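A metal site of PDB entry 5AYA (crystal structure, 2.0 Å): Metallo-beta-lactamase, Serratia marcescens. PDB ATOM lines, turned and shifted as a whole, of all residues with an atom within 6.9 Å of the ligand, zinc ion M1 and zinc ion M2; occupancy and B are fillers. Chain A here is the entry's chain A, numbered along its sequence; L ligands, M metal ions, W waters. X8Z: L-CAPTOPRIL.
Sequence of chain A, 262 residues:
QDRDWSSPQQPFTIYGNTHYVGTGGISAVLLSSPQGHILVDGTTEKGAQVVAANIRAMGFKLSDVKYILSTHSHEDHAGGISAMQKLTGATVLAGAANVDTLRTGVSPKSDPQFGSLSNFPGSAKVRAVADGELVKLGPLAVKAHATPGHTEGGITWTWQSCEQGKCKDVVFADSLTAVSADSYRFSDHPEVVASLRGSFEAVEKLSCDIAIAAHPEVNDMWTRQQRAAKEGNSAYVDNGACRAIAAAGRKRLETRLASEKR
Zinc ion M2 is bound by OD2 of Asp 76 (2.0 Å), NE2 of His 77 (2.1 Å), NE2 of His 215 (2.2 Å) and S of the ligand (2.4 Å). Zinc ion M2 has four donor atoms within binding distance.
The nearest printed residue that does not touch zinc ion M1 is His 77 (4.2 Å).
Three residues have an atom within 4 Å of zinc ion M2: Asp 76, His 77 and His 215. The nearest printed residue that does not touch zinc ion M2 is Ile 26 (4.3 Å).
Zinc ion M1 is bound by a ring nitrogen (NE2) of His 150, a ring nitrogen (ND1) of His 74, a ring nitrogen (NE2) of His 72 and a sulfur (S) of the ligand. Zinc ion M1 has four donor atoms within binding distance.
OG of Ser 175 touches C1 of the ligand (3.8 Å). Val 179 touches the ligand (CG2 to C3, 3.8 Å). OE2 of Glu 217 touches C7 of the ligand (3.5 Å). Within 4 Å of the ligand: His 72, His 74, Asp 76, His 77, His 150, Ser 175, Thr 177, Val 179, His 215, Glu 217 and Arg 252. Along chain A the residues within 4 Å of the ligand span positions 72 to 252. The nearest printed residue that does not touch the ligand is Gln 113 (4.1 Å).
An oxygen (O3) of the ligand lies within salt-bridge range of the guanidinium group (NH2) of Arg 252 (3.0 Å). The side-chain hydroxyl (OG1) of Thr 177 is in hydrogen-bond range of an oxygen (O1) of the ligand.
The backbone carbonyl oxygen (O) of Thr 177 lies within hydrogen-bond range of a ring nitrogen (ND1) of His 150, at 2.7 Å. The side-chain carboxylate (OD1) of Asp 174 sits at hydrogen-bond distance from a ring nitrogen (ND1) of His 72, 2.5 Å away. A ring nitrogen (NE2) of His 74 sits at hydrogen-bond distance from the side-chain carboxylate (OD2) of Asp 111, at 2.7 Å.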
ATOM      1  N   TRP A   5      15.487  37.436  32.229  1.00  0.00           N
ATOM      2  CA  TRP A   5      16.664  37.201  31.422  1.00  0.00           C
ATOM      3  C   TRP A   5      17.076  38.450  30.615  1.00  0.00           C
ATOM      4  O   TRP A   5      18.228  38.553  30.181  1.00  0.00           O
ATOM      5  CB  TRP A   5      16.424  36.023  30.455  1.00  0.00           C
ATOM      6  CG  TRP A   5      16.143  34.689  31.139  1.00  0.00           C
ATOM      7  CD1 TRP A   5      16.376  34.358  32.458  1.00  0.00           C
ATOM      8  CD2 TRP A   5      15.641  33.495  30.513  1.00  0.00           C
ATOM      9  NE1 TRP A   5      16.036  33.040  32.684  1.00  0.00           N
ATOM     10  CE2 TRP A   5      15.590  32.483  31.511  1.00  0.00           C
ATOM     11  CE3 TRP A   5      15.230  33.178  29.210  1.00  0.00           C
ATOM     12  CZ2 TRP A   5      15.144  31.189  31.245  1.00  0.00           C
ATOM     13  CZ3 TRP A   5      14.773  31.879  28.948  1.00  0.00           C
ATOM     14  CH2 TRP A   5      14.716  30.908  29.975  1.00  0.00           C
ATOM     15  N   ILE A  26      20.839  36.552  33.594  1.00  0.00           N
ATOM     16  CA  ILE A  26      21.835  35.794  32.818  1.00  0.00           C
ATOM     17  C   ILE A  26      23.195  36.479  32.863  1.00  0.00           C
ATOM     18  O   ILE A  26      23.279  37.673  32.638  1.00  0.00           O
ATOM     19  CB  ILE A  26      21.415  35.681  31.336  1.00  0.00           C
ATOM     20  CG1 ILE A  26      20.062  34.979  31.203  1.00  0.00           C
ATOM     21  CG2 ILE A  26      22.475  34.936  30.521  1.00  0.00           C
ATOM     22  CD1 ILE A  26      20.126  33.481  31.396  1.00  0.00           C
ATOM     23  N   HIS A  72      26.873  28.409  25.267  1.00  0.00           N
ATOM     24  CA  HIS A  72      26.042  27.587  24.367  1.00  0.00           C
ATOM     25  C   HIS A  72      24.855  28.319  23.727  1.00  0.00           C
ATOM     26  O   HIS A  72      24.436  29.395  24.195  1.00  0.00           O
ATOM     27  CB  HIS A  72      25.546  26.357  25.115  1.00  0.00           C
ATOM     28  CG  HIS A  72      24.475  26.645  26.101  1.00  0.00           C
ATOM     29  ND1 HIS A  72      24.735  26.906  27.437  1.00  0.00           N
ATOM     30  CD2 HIS A  72      23.136  26.739  25.955  1.00  0.00           C
ATOM     31  CE1 HIS A  72      23.605  27.197  28.051  1.00  0.00           C
ATOM     32  NE2 HIS A  72      22.618  27.074  27.177  1.00  0.00           N
ATOM     33  N   SER A  73      24.240  27.657  22.749  1.00  0.00           N
ATOM     34  CA  SER A  73      23.421  28.339  21.730  1.00  0.00           C
ATOM     35  C   SER A  73      21.942  28.178  22.011  1.00  0.00           C
ATOM     36  O   SER A  73      21.178  27.744  21.152  1.00  0.00           O
ATOM     37  CB  SER A  73      23.744  27.773  20.337  1.00  0.00           C
ATOM     38  OG  SER A  73      23.754  26.357  20.346  1.00  0.00           O
ATOM     39  N   HIS A  74      21.545  28.436  23.254  1.00  0.00           N
ATOM     40  CA  HIS A  74      20.157  28.689  23.566  1.00  0.00           C
ATOM     41  C   HIS A  74      19.912  30.177  23.638  1.00  0.00           C
ATOM     42  O   HIS A  74      20.838  30.938  23.963  1.00  0.00           O
ATOM     43  CB  HIS A  74      19.784  28.069  24.889  1.00  0.00           C
ATOM     44  CG  HIS A  74      19.755  26.586  24.846  1.00  0.00           C
ATOM     45  ND1 HIS A  74      19.624  25.815  25.971  1.00  0.00           N
ATOM     46  CD2 HIS A  74      19.794  25.733  23.801  1.00  0.00           C
ATOM     47  CE1 HIS A  74      19.640  24.541  25.629  1.00  0.00           C
ATOM     48  NE2 HIS A  74      19.731  24.457  24.318  1.00  0.00           N
ATOM     49  N   GLU A  75      18.682  30.563  23.339  1.00  0.00           N
ATOM     50  CA  GLU A  75      18.281  31.958  23.135  1.00  0.00           C
ATOM     51  C   GLU A  75      18.694  32.900  24.279  1.00  0.00           C
ATOM     52  O   GLU A  75      19.183  34.019  24.043  1.00  0.00           O
ATOM     53  CB  GLU A  75      16.764  32.024  22.891  1.00  0.00           C
ATOM     54  CG  GLU A  75      15.918  31.498  24.055  1.00  0.00           C
ATOM     55  CD  GLU A  75      14.417  31.451  23.752  1.00  0.00           C
ATOM     56  OE1 GLU A  75      13.973  32.095  22.769  1.00  0.00           O
ATOM     57  OE2 GLU A  75      13.672  30.801  24.531  1.00  0.00           O
ATOM     58  N   ASP A  76      18.551  32.415  25.503  1.00  0.00           N
ATOM     59  CA  ASP A  76      18.794  33.204  26.696  1.00  0.00           C
ATOM     60  C   ASP A  76      20.278  33.600  26.939  1.00  0.00           C
ATOM     61  O   ASP A  76      20.521  34.545  27.703  1.00  0.00           O
ATOM     62  CB  ASP A  76      18.197  32.532  27.953  1.00  0.00           C
ATOM     63  CG  ASP A  76      18.762  31.148  28.231  1.00  0.00           C
ATOM     64  OD1 ASP A  76      19.143  30.425  27.268  1.00  0.00           O
ATOM     65  OD2 ASP A  76      18.713  30.737  29.404  1.00  0.00           O
ATOM     66  N   HIS A  77      21.225  32.923  26.282  1.00  0.00           N
ATOM     67  CA  HIS A  77      22.655  33.308  26.346  1.00  0.00           C
ATOM     68  C   HIS A  77      23.149  33.878  25.038  1.00  0.00           C
ATOM     69  O   HIS A  77      24.097  34.662  25.026  1.00  0.00           O
ATOM     70  CB  HIS A  77      23.525  32.093  26.676  1.00  0.00           C
ATOM     71  CG  HIS A  77      23.031  31.316  27.843  1.00  0.00           C
ATOM     72  ND1 HIS A  77      23.150  31.767  29.141  1.00  0.00           N
ATOM     73  CD2 HIS A  77      22.289  30.177  27.904  1.00  0.00           C
ATOM     74  CE1 HIS A  77      22.575  30.905  29.962  1.00  0.00           C
ATOM     75  NE2 HIS A  77      21.977  29.980  29.227  1.00  0.00           N
ATOM     76  N   ASP A 111      19.549  19.080  19.538  1.00  0.00           N
ATOM     77  CA  ASP A 111      19.483  19.868  20.768  1.00  0.00           C
ATOM     78  C   ASP A 111      18.327  19.392  21.660  1.00  0.00           C
ATOM     79  O   ASP A 111      17.196  19.192  21.199  1.00  0.00           O
ATOM     80  CB  ASP A 111      19.312  21.349  20.431  1.00  0.00           C
ATOM     81  CG  ASP A 111      19.768  22.266  21.566  1.00  0.00           C
ATOM     82  OD1 ASP A 111      20.977  22.569  21.628  1.00  0.00           O
ATOM     83  OD2 ASP A 111      18.934  22.652  22.410  1.00  0.00           O
ATOM     84  N   GLN A 113      16.589  21.036  23.577  1.00  0.00           N
ATOM     85  CA  GLN A 113      15.539  22.061  23.591  1.00  0.00           C
ATOM     86  C   GLN A 113      15.193  22.591  22.203  1.00  0.00           C
ATOM     87  O   GLN A 113      14.572  23.646  22.081  1.00  0.00           O
ATOM     88  CB  GLN A 113      15.950  23.212  24.506  1.00  0.00           C
ATOM     89  CG  GLN A 113      16.141  22.775  25.948  1.00  0.00           C
ATOM     90  CD  GLN A 113      16.386  23.939  26.881  1.00  0.00           C
ATOM     91  OE1 GLN A 113      15.975  25.063  26.609  1.00  0.00           O
ATOM     92  NE2 GLN A 113      17.117  23.694  27.950  1.00  0.00           N
ATOM     93  N   LEU A 117      12.642  25.700  22.984  1.00  0.00           N
ATOM     94  CA  LEU A 117      13.196  27.037  22.767  1.00  0.00           C
ATOM     95  C   LEU A 117      12.974  27.490  21.334  1.00  0.00           C
ATOM     96  O   LEU A 117      13.601  26.976  20.398  1.00  0.00           O
ATOM     97  CB  LEU A 117      14.696  27.070  23.073  1.00  0.00           C
ATOM     98  CG  LEU A 117      15.128  26.876  24.532  1.00  0.00           C
ATOM     99  CD1 LEU A 117      16.383  27.671  24.804  1.00  0.00           C
ATOM    100  CD2 LEU A 117      14.032  27.267  25.527  1.00  0.00           C
ATOM    101  N   HIS A 150      24.464  19.537  27.567  1.00  0.00           N
ATOM    102  CA  HIS A 150      23.298  20.407  27.584  1.00  0.00           C
ATOM    103  C   HIS A 150      23.077  20.875  26.148  1.00  0.00           C
ATOM    104  O   HIS A 150      21.937  21.077  25.722  1.00  0.00           O
ATOM    105  CB  HIS A 150      23.553  21.595  28.565  1.00  0.00           C
ATOM    106  CG  HIS A 150      22.452  22.612  28.644  1.00  0.00           C
ATOM    107  ND1 HIS A 150      21.475  22.549  29.611  1.00  0.00           N
ATOM    108  CD2 HIS A 150      22.282  23.799  28.015  1.00  0.00           C
ATOM    109  CE1 HIS A 150      20.687  23.604  29.509  1.00  0.00           C
ATOM    110  NE2 HIS A 150      21.149  24.385  28.551  1.00  0.00           N
ATOM    111  N   THR A 151      24.196  21.139  25.464  1.00  0.00           N
ATOM    112  CA  THR A 151      24.242  21.303  24.014  1.00  0.00           C
ATOM    113  C   THR A 151      25.494  20.568  23.542  1.00  0.00           C
ATOM    114  O   THR A 151      26.406  20.320  24.349  1.00  0.00           O
ATOM    115  CB  THR A 151      24.372  22.767  23.550  1.00  0.00           C
ATOM    116  OG1 THR A 151      25.639  23.290  23.979  1.00  0.00           O
ATOM    117  CG2 THR A 151      23.219  23.649  24.089  1.00  0.00           C
ATOM    118  N   ASP A 174      29.699  26.925  31.705  1.00  0.00           N
ATOM    119  CA  ASP A 174      28.537  26.614  30.883  1.00  0.00           C
ATOM    120  C   ASP A 174      27.546  25.812  31.708  1.00  0.00           C
ATOM    121  O   ASP A 174      27.909  25.233  32.725  1.00  0.00           O
ATOM    122  CB  ASP A 174      28.953  25.805  29.660  1.00  0.00           C
ATOM    123  CG  ASP A 174      27.912  25.851  28.527  1.00  0.00           C
ATOM    124  OD1 ASP A 174      26.982  26.690  28.600  1.00  0.00           O
ATOM    125  OD2 ASP A 174      27.979  24.997  27.638  1.00  0.00           O
ATOM    126  N   SER A 175      26.278  25.789  31.259  1.00  0.00           N
ATOM    127  CA  SER A 175      25.253  24.980  31.924  1.00  0.00           C
ATOM    128  C   SER A 175      25.552  23.512  31.731  1.00  0.00           C
ATOM    129  O   SER A 175      25.866  23.057  30.619  1.00  0.00           O
ATOM    130  CB  SER A 175      23.836  25.299  31.399  1.00  0.00           C
ATOM    131  OG  SER A 175      23.654  26.700  31.253  1.00  0.00           O
ATOM    132  N   LEU A 176      25.392  22.754  32.811  1.00  0.00           N
ATOM    133  CA  LEU A 176      25.593  21.307  32.830  1.00  0.00           C
ATOM    134  C   LEU A 176      24.280  20.571  33.168  1.00  0.00           C
ATOM    135  O   LEU A 176      24.304  19.393  33.566  1.00  0.00           O
ATOM    136  CB  LEU A 176      26.658  20.969  33.864  1.00  0.00           C
ATOM    137  CG  LEU A 176      28.031  21.675  33.676  1.00  0.00           C
ATOM    138  CD1 LEU A 176      28.938  21.361  34.861  1.00  0.00           C
ATOM    139  CD2 LEU A 176      28.668  21.248  32.364  1.00  0.00           C
ATOM    140  N   THR A 177      23.165  21.206  32.860  1.00  0.00           N
ATOM    141  CA  THR A 177      21.842  20.724  33.248  1.00  0.00           C
ATOM    142  C   THR A 177      21.203  19.842  32.166  1.00  0.00           C
ATOM    143  O   THR A 177      21.143  20.216  30.979  1.00  0.00           O
ATOM    144  CB  THR A 177      20.904  21.895  33.626  1.00  0.00           C
ATOM    145  OG1 THR A 177      20.974  22.956  32.663  1.00  0.00           O
ATOM    146  CG2 THR A 177      21.286  22.433  34.995  1.00  0.00           C
ATOM    147  N   VAL A 179      18.261  19.202  30.740  1.00  0.00           N
ATOM    148  CA  VAL A 179      16.913  19.685  30.518  1.00  0.00           C
ATOM    149  C   VAL A 179      16.690  19.776  29.032  1.00  0.00           C
ATOM    150  O   VAL A 179      17.636  19.871  28.269  1.00  0.00           O
ATOM    151  CB  VAL A 179      16.675  21.064  31.158  1.00  0.00           C
ATOM    152  CG1 VAL A 179      16.538  20.934  32.667  1.00  0.00           C
ATOM    153  CG2 VAL A 179      17.791  22.031  30.804  1.00  0.00           C
ATOM    154  N   ALA A 214      26.679  30.530  33.992  1.00  0.00           N
ATOM    155  CA  ALA A 214      25.902  31.188  32.934  1.00  0.00           C
ATOM    156  C   ALA A 214      24.587  31.708  33.517  1.00  0.00           C
ATOM    157  O   ALA A 214      24.217  32.873  33.320  1.00  0.00           O
ATOM    158  CB  ALA A 214      25.641  30.208  31.791  1.00  0.00           C
ATOM    159  N   HIS A 215      23.912  30.842  34.269  1.00  0.00           N
ATOM    160  CA  HIS A 215      22.891  31.289  35.227  1.00  0.00           C
ATOM    161  C   HIS A 215      23.527  31.648  36.585  1.00  0.00           C
ATOM    162  O   HIS A 215      23.928  30.778  37.362  1.00  0.00           O
ATOM    163  CB  HIS A 215      21.795  30.219  35.381  1.00  0.00           C
ATOM    164  CG  HIS A 215      20.933  30.056  34.156  1.00  0.00           C
ATOM    165  ND1 HIS A 215      19.920  30.929  33.826  1.00  0.00           N
ATOM    166  CD2 HIS A 215      21.021  29.170  33.137  1.00  0.00           C
ATOM    167  CE1 HIS A 215      19.407  30.582  32.657  1.00  0.00           C
ATOM    168  NE2 HIS A 215      20.056  29.520  32.213  1.00  0.00           N
ATOM    169  N   GLU A 217      22.889  32.689  39.583  1.00  0.00           N
ATOM    170  CA  GLU A 217      22.541  32.137  40.889  1.00  0.00           C
ATOM    171  C   GLU A 217      23.098  30.732  41.136  1.00  0.00           C
ATOM    172  O   GLU A 217      23.246  30.328  42.288  1.00  0.00           O
ATOM    173  CB  GLU A 217      21.020  32.156  41.091  1.00  0.00           C
ATOM    174  CG  GLU A 217      20.241  31.049  40.401  1.00  0.00           C
ATOM    175  CD  GLU A 217      20.081  31.276  38.919  1.00  0.00           C
ATOM    176  OE1 GLU A 217      20.313  32.414  38.455  1.00  0.00           O
ATOM    177  OE2 GLU A 217      19.736  30.308  38.215  1.00  0.00           O
ATOM    178  N   VAL A 218      23.540  30.049  40.083  1.00  0.00           N
ATOM    179  CA  VAL A 218      24.043  28.690  40.224  1.00  0.00           C
ATOM    180  C   VAL A 218      25.352  28.669  41.020  1.00  0.00           C
ATOM    181  O   VAL A 218      25.711  27.625  41.592  1.00  0.00           O
ATOM    182  CB  VAL A 218      24.279  28.027  38.836  1.00  0.00           C
ATOM    183  CG1 VAL A 218      24.940  26.665  38.978  1.00  0.00           C
ATOM    184  CG2 VAL A 218      22.954  27.889  38.073  1.00  0.00           C
ATOM    185  N   ARG A 252      21.390  16.401  39.001  1.00  0.00           N
ATOM    186  CA  ARG A 252      20.296  16.740  38.123  1.00  0.00           C
ATOM    187  C   ARG A 252      20.101  15.700  37.014  1.00  0.00           C
ATOM    188  O   ARG A 252      18.975  15.436  36.600  1.00  0.00           O
ATOM    189  CB  ARG A 252      20.531  18.124  37.510  1.00  0.00           C
ATOM    190  CG  ARG A 252      19.394  18.608  36.631  1.00  0.00           C
ATOM    191  CD  ARG A 252      18.114  18.842  37.422  1.00  0.00           C
ATOM    192  NE  ARG A 252      17.290  19.851  36.768  1.00  0.00           N
ATOM    193  CZ  ARG A 252      17.540  21.159  36.783  1.00  0.00           C
ATOM    194  NH1 ARG A 252      18.545  21.643  37.514  1.00  0.00           N
ATOM    195  NH2 ARG A 252      16.769  21.994  36.090  1.00  0.00           N
HETATM  196  O1  X8Z L   1      20.133  25.546  33.435  1.00  0.00           O
HETATM  197  C4  X8Z L   1      19.184  26.311  33.305  1.00  0.00           C
HETATM  198  C2  X8Z L   1      18.688  26.634  31.913  1.00  0.00           C
HETATM  199  C1  X8Z L   1      19.856  26.467  30.970  1.00  0.00           C
HETATM  200  S   X8Z L   1      19.541  27.201  29.371  1.00  0.00           S
HETATM  201  C3  X8Z L   1      17.479  25.782  31.498  1.00  0.00           C
HETATM  202  N   X8Z L   1      18.569  26.953  34.310  1.00  0.00           N
HETATM  203  C8  X8Z L   1      19.076  26.886  35.688  1.00  0.00           C
HETATM  204  C9  X8Z L   1      19.072  25.501  36.244  1.00  0.00           C
HETATM  205  O3  X8Z L   1      18.072  24.690  35.913  1.00  0.00           O
HETATM  206  O2  X8Z L   1      19.927  25.153  37.045  1.00  0.00           O
HETATM  207  C5  X8Z L   1      17.382  27.806  34.197  1.00  0.00           C
HETATM  208  C6  X8Z L   1      17.116  28.370  35.591  1.00  0.00           C
HETATM  209  C7  X8Z L   1      18.122  27.728  36.531  1.00  0.00           C
HETATM  210 ZN    ZN M   1      20.728  26.199  27.742  1.00  0.00          ZN
HETATM  211 ZN    ZN M   2      20.144  29.410  29.969  1.00  0.00          ZN
HETATM  212  O   HOH W   1      22.570  25.821  34.938  1.00  0.00           O
